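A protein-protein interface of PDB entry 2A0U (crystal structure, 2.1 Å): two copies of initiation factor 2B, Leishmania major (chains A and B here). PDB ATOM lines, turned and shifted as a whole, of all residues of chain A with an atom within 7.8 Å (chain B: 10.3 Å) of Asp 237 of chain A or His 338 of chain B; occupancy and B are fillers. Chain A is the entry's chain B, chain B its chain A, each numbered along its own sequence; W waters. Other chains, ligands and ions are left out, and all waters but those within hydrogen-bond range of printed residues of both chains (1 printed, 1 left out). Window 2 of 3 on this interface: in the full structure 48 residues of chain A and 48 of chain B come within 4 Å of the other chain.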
ATOM      1  N   PHE A 206      13.709  -0.524  -8.420  1.00  0.00           N
ATOM      2  CA  PHE A 206      13.935  -0.457  -9.865  1.00  0.00           C
ATOM      3  C   PHE A 206      15.179   0.361 -10.231  1.00  0.00           C
ATOM      4  O   PHE A 206      15.944  -0.036 -11.115  1.00  0.00           O
ATOM      5  CB  PHE A 206      12.689   0.087 -10.580  1.00  0.00           C
ATOM      6  CG  PHE A 206      12.914   0.442 -12.025  1.00  0.00           C
ATOM      7  CD1 PHE A 206      13.108  -0.551 -12.982  1.00  0.00           C
ATOM      8  CD2 PHE A 206      12.920   1.774 -12.432  1.00  0.00           C
ATOM      9  CE1 PHE A 206      13.314  -0.222 -14.320  1.00  0.00           C
ATOM     10  CE2 PHE A 206      13.122   2.113 -13.767  1.00  0.00           C
ATOM     11  CZ  PHE A 206      13.319   1.113 -14.714  1.00  0.00           C
ATOM     12  N   LEU A 211      14.843  -4.801  -8.979  1.00  0.00           N
ATOM     13  CA  LEU A 211      13.459  -5.209  -9.214  1.00  0.00           C
ATOM     14  C   LEU A 211      13.336  -6.110 -10.440  1.00  0.00           C
ATOM     15  O   LEU A 211      13.690  -5.717 -11.554  1.00  0.00           O
ATOM     16  CB  LEU A 211      12.547  -3.983  -9.356  1.00  0.00           C
ATOM     17  CG  LEU A 211      11.045  -4.230  -9.540  1.00  0.00           C
ATOM     18  CD1 LEU A 211      10.342  -4.486  -8.209  1.00  0.00           C
ATOM     19  CD2 LEU A 211      10.407  -3.066 -10.271  1.00  0.00           C
ATOM     20  N   GLU A 212      12.836  -7.323 -10.223  1.00  0.00           N
ATOM     21  CA  GLU A 212      12.539  -8.229 -11.323  1.00  0.00           C
ATOM     22  C   GLU A 212      11.228  -7.827 -11.991  1.00  0.00           C
ATOM     23  O   GLU A 212      11.163  -7.707 -13.218  1.00  0.00           O
ATOM     24  CB  GLU A 212      12.476  -9.683 -10.849  1.00  0.00           C
ATOM     25  CG  GLU A 212      12.328 -10.689 -11.992  1.00  0.00           C
ATOM     26  CD  GLU A 212      12.308 -12.135 -11.528  1.00  0.00           C
ATOM     27  OE1 GLU A 212      11.986 -12.390 -10.347  1.00  0.00           O
ATOM     28  OE2 GLU A 212      12.610 -13.022 -12.356  1.00  0.00           O
ATOM     29  N   ARG A 213      10.195  -7.607 -11.177  1.00  0.00           N
ATOM     30  CA  ARG A 213       8.854  -7.315 -11.677  1.00  0.00           C
ATOM     31  C   ARG A 213       7.927  -6.817 -10.574  1.00  0.00           C
ATOM     32  O   ARG A 213       7.978  -7.299  -9.440  1.00  0.00           O
ATOM     33  CB  ARG A 213       8.257  -8.571 -12.318  1.00  0.00           C
ATOM     34  CG  ARG A 213       7.058  -8.330 -13.214  1.00  0.00           C
ATOM     35  CD  ARG A 213       6.915  -9.447 -14.233  1.00  0.00           C
ATOM     36  NE  ARG A 213       7.947  -9.382 -15.268  1.00  0.00           N
ATOM     37  CZ  ARG A 213       7.858  -8.662 -16.384  1.00  0.00           C
ATOM     38  NH1 ARG A 213       6.780  -7.929 -16.635  1.00  0.00           N
ATOM     39  NH2 ARG A 213       8.856  -8.674 -17.256  1.00  0.00           N
ATOM     40  N   VAL A 214       7.086  -5.845 -10.915  1.00  0.00           N
ATOM     41  CA  VAL A 214       5.953  -5.484 -10.071  1.00  0.00           C
ATOM     42  C   VAL A 214       4.669  -6.042 -10.690  1.00  0.00           C
ATOM     43  O   VAL A 214       4.393  -5.824 -11.871  1.00  0.00           O
ATOM     44  CB  VAL A 214       5.865  -3.946  -9.794  1.00  0.00           C
ATOM     45  CG1 VAL A 214       5.735  -3.135 -11.088  1.00  0.00           C
ATOM     46  CG2 VAL A 214       4.725  -3.625  -8.824  1.00  0.00           C
ATOM     47  N   VAL A 230      -0.301   0.958 -13.968  1.00  0.00           N
ATOM     48  CA  VAL A 230       0.281   0.508 -15.235  1.00  0.00           C
ATOM     49  C   VAL A 230       0.855   1.703 -16.003  1.00  0.00           C
ATOM     50  O   VAL A 230       1.990   1.648 -16.488  1.00  0.00           O
ATOM     51  CB  VAL A 230      -0.746  -0.269 -16.099  1.00  0.00           C
ATOM     52  CG1 VAL A 230      -0.257  -0.420 -17.536  1.00  0.00           C
ATOM     53  CG2 VAL A 230      -1.038  -1.634 -15.485  1.00  0.00           C
ATOM     54  N   TYR A 231       0.072   2.779 -16.083  1.00  0.00           N
ATOM     55  CA  TYR A 231       0.492   4.026 -16.728  1.00  0.00           C
ATOM     56  C   TYR A 231       1.821   4.552 -16.175  1.00  0.00           C
ATOM     57  O   TYR A 231       2.719   4.898 -16.943  1.00  0.00           O
ATOM     58  CB  TYR A 231      -0.608   5.090 -16.603  1.00  0.00           C
ATOM     59  CG  TYR A 231      -0.289   6.416 -17.263  1.00  0.00           C
ATOM     60  CD1 TYR A 231      -0.368   6.570 -18.650  1.00  0.00           C
ATOM     61  CD2 TYR A 231       0.078   7.521 -16.501  1.00  0.00           C
ATOM     62  CE1 TYR A 231      -0.079   7.793 -19.257  1.00  0.00           C
ATOM     63  CE2 TYR A 231       0.370   8.747 -17.100  1.00  0.00           C
ATOM     64  CZ  TYR A 231       0.291   8.875 -18.473  1.00  0.00           C
ATOM     65  OH  TYR A 231       0.581  10.090 -19.056  1.00  0.00           O
ATOM     66  N   GLU A 232       1.941   4.605 -14.848  1.00  0.00           N
ATOM     67  CA  GLU A 232       3.167   5.074 -14.194  1.00  0.00           C
ATOM     68  C   GLU A 232       4.376   4.193 -14.524  1.00  0.00           C
ATOM     69  O   GLU A 232       5.466   4.705 -14.787  1.00  0.00           O
ATOM     70  CB  GLU A 232       2.981   5.176 -12.672  1.00  0.00           C
ATOM     71  CG  GLU A 232       2.147   6.371 -12.213  1.00  0.00           C
ATOM     72  CD  GLU A 232       2.278   6.656 -10.724  1.00  0.00           C
ATOM     73  OE1 GLU A 232       3.416   6.836 -10.239  1.00  0.00           O
ATOM     74  OE2 GLU A 232       1.238   6.720 -10.035  1.00  0.00           O
ATOM     75  N   CYS A 233       4.172   2.876 -14.518  1.00  0.00           N
ATOM     76  CA  CYS A 233       5.228   1.915 -14.839  1.00  0.00           C
ATOM     77  C   CYS A 233       5.675   1.993 -16.300  1.00  0.00           C
ATOM     78  O   CYS A 233       6.858   1.816 -16.601  1.00  0.00           O
ATOM     79  CB  CYS A 233       4.781   0.491 -14.501  1.00  0.00           C
ATOM     80  SG  CYS A 233       4.640   0.157 -12.733  1.00  0.00           S
ATOM     81  N   VAL A 234       4.727   2.258 -17.197  1.00  0.00           N
ATOM     82  CA  VAL A 234       5.014   2.398 -18.627  1.00  0.00           C
ATOM     83  C   VAL A 234       5.870   3.638 -18.906  1.00  0.00           C
ATOM     84  O   VAL A 234       6.843   3.571 -19.660  1.00  0.00           O
ATOM     85  CB  VAL A 234       3.708   2.419 -19.473  1.00  0.00           C
ATOM     86  CG1 VAL A 234       3.974   2.912 -20.889  1.00  0.00           C
ATOM     87  CG2 VAL A 234       3.082   1.034 -19.515  1.00  0.00           C
ATOM     88  N   GLN A 235       5.514   4.757 -18.276  1.00  0.00           N
ATOM     89  CA  GLN A 235       6.228   6.024 -18.466  1.00  0.00           C
ATOM     90  C   GLN A 235       7.684   5.975 -17.991  1.00  0.00           C
ATOM     91  O   GLN A 235       8.524   6.730 -18.486  1.00  0.00           O
ATOM     92  CB  GLN A 235       5.488   7.184 -17.785  1.00  0.00           C
ATOM     93  CG  GLN A 235       4.094   7.494 -18.343  1.00  0.00           C
ATOM     94  CD  GLN A 235       4.109   7.968 -19.789  1.00  0.00           C
ATOM     95  OE1 GLN A 235       4.274   7.175 -20.718  1.00  0.00           O
ATOM     96  NE2 GLN A 235       3.917   9.267 -19.986  1.00  0.00           N
ATOM     97  N   GLU A 236       7.975   5.085 -17.044  1.00  0.00           N
ATOM     98  CA  GLU A 236       9.325   4.950 -16.491  1.00  0.00           C
ATOM     99  C   GLU A 236      10.016   3.627 -16.852  1.00  0.00           C
ATOM    100  O   GLU A 236      11.095   3.327 -16.331  1.00  0.00           O
ATOM    101  CB  GLU A 236       9.307   5.149 -14.969  1.00  0.00           C
ATOM    102  CG  GLU A 236       9.045   6.586 -14.529  1.00  0.00           C
ATOM    103  CD  GLU A 236       9.307   6.818 -13.048  1.00  0.00           C
ATOM    104  OE1 GLU A 236      10.293   6.267 -12.512  1.00  0.00           O
ATOM    105  OE2 GLU A 236       8.529   7.568 -12.423  1.00  0.00           O
ATOM    106  N   ASP A 237       9.395   2.852 -17.743  1.00  0.00           N
ATOM    107  CA  ASP A 237       9.933   1.562 -18.212  1.00  0.00           C
ATOM    108  C   ASP A 237      10.117   0.530 -17.093  1.00  0.00           C
ATOM    109  O   ASP A 237      10.970  -0.356 -17.188  1.00  0.00           O
ATOM    110  CB  ASP A 237      11.254   1.757 -18.974  1.00  0.00           C
ATOM    111  CG  ASP A 237      11.103   2.633 -20.202  1.00  0.00           C
ATOM    112  OD1 ASP A 237      10.287   2.294 -21.085  1.00  0.00           O
ATOM    113  OD2 ASP A 237      11.820   3.653 -20.291  1.00  0.00           O
ATOM    114  N   ILE A 238       9.316   0.652 -16.036  1.00  0.00           N
ATOM    115  CA  ILE A 238       9.349  -0.287 -14.917  1.00  0.00           C
ATOM    116  C   ILE A 238       8.658  -1.591 -15.328  1.00  0.00           C
ATOM    117  O   ILE A 238       7.478  -1.574 -15.688  1.00  0.00           O
ATOM    118  CB  ILE A 238       8.667   0.304 -13.653  1.00  0.00           C
ATOM    119  CG1 ILE A 238       9.341   1.618 -13.238  1.00  0.00           C
ATOM    120  CG2 ILE A 238       8.688  -0.704 -12.504  1.00  0.00           C
ATOM    121  CD1 ILE A 238       8.519   2.473 -12.283  1.00  0.00           C
ATOM    122  N   PRO A 239       9.397  -2.722 -15.290  1.00  0.00           N
ATOM    123  CA  PRO A 239       8.825  -4.028 -15.629  1.00  0.00           C
ATOM    124  C   PRO A 239       7.583  -4.329 -14.791  1.00  0.00           C
ATOM    125  O   PRO A 239       7.663  -4.419 -13.562  1.00  0.00           O
ATOM    126  CB  PRO A 239       9.961  -5.016 -15.315  1.00  0.00           C
ATOM    127  CG  PRO A 239      10.947  -4.247 -14.491  1.00  0.00           C
ATOM    128  CD  PRO A 239      10.823  -2.830 -14.933  1.00  0.00           C
ATOM    129  N   CYS A 240       6.447  -4.464 -15.470  1.00  0.00           N
ATOM    130  CA  CYS A 240       5.149  -4.560 -14.814  1.00  0.00           C
ATOM    131  C   CYS A 240       4.276  -5.641 -15.438  1.00  0.00           C
ATOM    132  O   CYS A 240       4.304  -5.849 -16.654  1.00  0.00           O
ATOM    133  CB  CYS A 240       4.434  -3.206 -14.879  1.00  0.00           C
ATOM    134  SG  CYS A 240       2.747  -3.193 -14.228  1.00  0.00           S
ATOM    135  N   THR A 241       3.506  -6.324 -14.597  1.00  0.00           N
ATOM    136  CA  THR A 241       2.533  -7.307 -15.061  1.00  0.00           C
ATOM    137  C   THR A 241       1.170  -7.052 -14.427  1.00  0.00           C
ATOM    138  O   THR A 241       1.029  -7.065 -13.201  1.00  0.00           O
ATOM    139  CB  THR A 241       2.999  -8.753 -14.796  1.00  0.00           C
ATOM    140  OG1 THR A 241       4.193  -9.010 -15.543  1.00  0.00           O
ATOM    141  CG2 THR A 241       1.930  -9.761 -15.207  1.00  0.00           C
ATOM    142  N   ARG B 331      -8.885   0.984 -25.737  1.00  0.00           N
ATOM    143  CA  ARG B 331      -7.848   0.373 -24.912  1.00  0.00           C
ATOM    144  C   ARG B 331      -7.739   1.149 -23.606  1.00  0.00           C
ATOM    145  O   ARG B 331      -7.110   2.209 -23.544  1.00  0.00           O
ATOM    146  CB  ARG B 331      -6.497   0.311 -25.633  1.00  0.00           C
ATOM    147  CG  ARG B 331      -5.501  -0.599 -24.924  1.00  0.00           C
ATOM    148  CD  ARG B 331      -4.080  -0.424 -25.422  1.00  0.00           C
ATOM    149  NE  ARG B 331      -3.115  -0.827 -24.398  1.00  0.00           N
ATOM    150  CZ  ARG B 331      -2.662  -2.067 -24.219  1.00  0.00           C
ATOM    151  NH1 ARG B 331      -3.072  -3.058 -25.003  1.00  0.00           N
ATOM    152  NH2 ARG B 331      -1.790  -2.316 -23.251  1.00  0.00           N
ATOM    153  N   ALA B 334      -2.867   1.638 -20.495  1.00  0.00           N
ATOM    154  CA  ALA B 334      -1.695   2.156 -21.205  1.00  0.00           C
ATOM    155  C   ALA B 334      -0.824   1.016 -21.735  1.00  0.00           C
ATOM    156  O   ALA B 334      -0.843  -0.091 -21.194  1.00  0.00           O
ATOM    157  CB  ALA B 334      -0.883   3.067 -20.299  1.00  0.00           C
ATOM    158  N   ASP B 335      -0.068   1.287 -22.797  1.00  0.00           N
ATOM    159  CA  ASP B 335       0.784   0.271 -23.412  1.00  0.00           C
ATOM    160  C   ASP B 335       2.254   0.682 -23.445  1.00  0.00           C
ATOM    161  O   ASP B 335       2.581   1.847 -23.679  1.00  0.00           O
ATOM    162  CB  ASP B 335       0.297  -0.061 -24.828  1.00  0.00           C
ATOM    163  CG  ASP B 335       0.888  -1.359 -25.366  1.00  0.00           C
ATOM    164  OD1 ASP B 335       1.253  -2.244 -24.561  1.00  0.00           O
ATOM    165  OD2 ASP B 335       0.979  -1.496 -26.604  1.00  0.00           O
ATOM    166  N   GLY B 336       3.131  -0.292 -23.214  1.00  0.00           N
ATOM    167  CA  GLY B 336       4.574  -0.072 -23.223  1.00  0.00           C
ATOM    168  C   GLY B 336       5.359  -1.355 -23.437  1.00  0.00           C
ATOM    169  O   GLY B 336       4.814  -2.449 -23.271  1.00  0.00           O
ATOM    170  N   PRO B 337       6.648  -1.233 -23.814  1.00  0.00           N
ATOM    171  CA  PRO B 337       7.510  -2.396 -24.067  1.00  0.00           C
ATOM    172  C   PRO B 337       7.814  -3.254 -22.834  1.00  0.00           C
ATOM    173  O   PRO B 337       8.129  -4.437 -22.979  1.00  0.00           O
ATOM    174  CB  PRO B 337       8.801  -1.769 -24.612  1.00  0.00           C
ATOM    175  CG  PRO B 337       8.799  -0.378 -24.097  1.00  0.00           C
ATOM    176  CD  PRO B 337       7.361   0.036 -24.052  1.00  0.00           C
ATOM    177  N   HIS B 338       7.721  -2.666 -21.641  1.00  0.00           N
ATOM    178  CA  HIS B 338       8.033  -3.378 -20.399  1.00  0.00           C
ATOM    179  C   HIS B 338       6.780  -3.709 -19.581  1.00  0.00           C
ATOM    180  O   HIS B 338       6.839  -3.866 -18.359  1.00  0.00           O
ATOM    181  CB  HIS B 338       9.043  -2.582 -19.565  1.00  0.00           C
ATOM    182  CG  HIS B 338      10.327  -2.301 -20.283  1.00  0.00           C
ATOM    183  ND1 HIS B 338      10.551  -1.130 -20.975  1.00  0.00           N
ATOM    184  CD2 HIS B 338      11.449  -3.044 -20.427  1.00  0.00           C
ATOM    185  CE1 HIS B 338      11.759  -1.162 -21.508  1.00  0.00           C
ATOM    186  NE2 HIS B 338      12.325  -2.312 -21.191  1.00  0.00           N
ATOM    187  N   LEU B 339       5.651  -3.811 -20.276  1.00  0.00           N
ATOM    188  CA  LEU B 339       4.392  -4.218 -19.672  1.00  0.00           C
ATOM    189  C   LEU B 339       3.952  -5.562 -20.238  1.00  0.00           C
ATOM    190  O   LEU B 339       3.994  -5.775 -21.452  1.00  0.00           O
ATOM    191  CB  LEU B 339       3.309  -3.166 -19.931  1.00  0.00           C
ATOM    192  CG  LEU B 339       1.872  -3.542 -19.552  1.00  0.00           C
ATOM    193  CD1 LEU B 339       1.656  -3.459 -18.043  1.00  0.00           C
ATOM    194  CD2 LEU B 339       0.884  -2.670 -20.295  1.00  0.00           C
ATOM    195  N   SER B 340       3.536  -6.463 -19.354  1.00  0.00           N
ATOM    196  CA  SER B 340       2.944  -7.728 -19.773  1.00  0.00           C
ATOM    197  C   SER B 340       1.618  -7.960 -19.057  1.00  0.00           C
ATOM    198  O   SER B 340       1.363  -7.389 -17.996  1.00  0.00           O
ATOM    199  CB  SER B 340       3.910  -8.899 -19.553  1.00  0.00           C
ATOM    200  OG  SER B 340       4.042  -9.216 -18.179  1.00  0.00           O
ATOM    201  N   ILE B 341       0.771  -8.787 -19.661  1.00  0.00           N
ATOM    202  CA  ILE B 341      -0.538  -9.100 -19.100  1.00  0.00           C
ATOM    203  C   ILE B 341      -0.615 -10.595 -18.821  1.00  0.00           C
ATOM    204  O   ILE B 341      -0.417 -11.408 -19.725  1.00  0.00           O
ATOM    205  CB  ILE B 341      -1.691  -8.683 -20.067  1.00  0.00           C
ATOM    206  CG1 ILE B 341      -1.521  -7.235 -20.565  1.00  0.00           C
ATOM    207  CG2 ILE B 341      -3.063  -8.914 -19.426  1.00  0.00           C
ATOM    208  CD1 ILE B 341      -1.520  -6.157 -19.479  1.00  0.00           C
HETATM  209  O   HOH W   1      -2.766   2.131 -17.574  1.00  0.00           O
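O of Ala 334 of chain B lies within hydrogen-bond range of NH2 of Arg 331 of chain B, 3.2 Å away.
NH1 of Arg 213 of chain A sits at hydrogen-bond distance from O of Cys 240 of chain A, 3.2 Å away.
NH1 of Arg 213 of chain A is in hydrogen-bond range of OG1 of Thr 241 of chain A (3.0 Å).
The backbone carbonyl oxygen (O) of Pro 239 of chain A is in hydrogen-bond range of the backbone NH (N) of Val 214 of chain A, 3.1 Å away.
N of Thr 241 of chain A sits at hydrogen-bond distance from O of Val 214 of chain A, at 2.9 Å.
N of Ile 238 of chain A is in hydrogen-bond range of O of Cys 233 of chain A (2.8 Å).
A ring nitrogen (ND1) of His 338 of chain B is in hydrogen-bond range of the side-chain carboxylate (OD1) of Asp 237 of chain A (3.4 Å).
N of Cys 240 of chain A is in hydrogen-bond range of O of His 338 of chain B (3.0 Å).
The side-chain hydroxyl (OG) of Ser 340 of chain B is in hydrogen-bond range of the guanidinium group (NH1) of Arg 213 of chain A.
The backbone NH of Ser 340 of chain B lies within hydrogen-bond range of the backbone carbonyl oxygen of Cys 240 of chain A.
The side-chain hydroxyl of Ser 340 of chain B is in hydrogen-bond range of the side-chain hydroxyl of Thr 241 of chain A (2.6 Å).
Water W1 bridges N of Ala 334 of chain B (3.0 Å) and N of Tyr 231 of chain A (3.3 Å).
Of chain B, only His 338 comes within 4 Å of Ile 238 of chain A.
Of chain B, only His 338 (3.4 Å) comes within 4 Å of Pro 239 of chain A.
Of chain B, only His 338 (3.0 Å), Leu 339 (3.4 Å) and Ser 340 (2.9 Å) come within 4 Å of Cys 240 of chain A.
No residue of chain A comes within 4 Å of Pro 337 of chain B.
Of the printed residues of chain A, Gly 336 of chain B touches Val 234.
Of the printed residues of chain A, Ala 334 of chain B touches Val 230 (3.7 Å) and Tyr 231 (3.9 Å).
Of the printed residues of chain B, Val 230 of chain A touches Ala 334 and Leu 339.
Of the printed residues of chain B, Arg 213 of chain A touches Ser 340 (3.4 Å).
Of the printed residues of chain A, Leu 339 of chain B touches Val 230 and Cys 240.
No position is printed for both chains.
Among the printed residues, pairs that only touch across the chains: Val 234 of chain A with Asp 335 of chain B (3.3 Å), Pro 239 of chain A with His 338 of chain B (3.4 Å), Cys 240 of chain A with Leu 339 of chain B (3.4 Å), Ile 238 of chain A with His 338 of chain B (3.6 Å), Val 230 of chain A with Leu 339 of chain B (3.6 Å), Val 230 of chain A with Ala 334 of chain B (3.7 Å), Val 234 of chain A with Gly 336 of chain B (3.8 Å) and Tyr 231 of chain A with Ala 334 of chain B (3.9 Å).
Of the 17 printed residues of chain A, 9 touch a printed residue of chain B.
Printed residues of chain A that touch a printed residue of chain B: Arg 213, Val 230, Tyr 231, Val 234, Asp 237, Ile 238, Pro 239, Cys 240 and Thr 241.
Hydrophobic or aromatic side chains of chain A that line the printed part of chain B: Val 230, Tyr 231 and Val 234.
Hydrophobic or aromatic side chains of chain B that line the printed part of chain A: Ala 334, His 338 and Leu 339.
Among the printed residues, 13 pairs touch across the chains.
Among the printed residues, no Asp or Glu carboxylate lies within 4 Å of a Lys or Arg side-chain nitrogen of the other chain.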
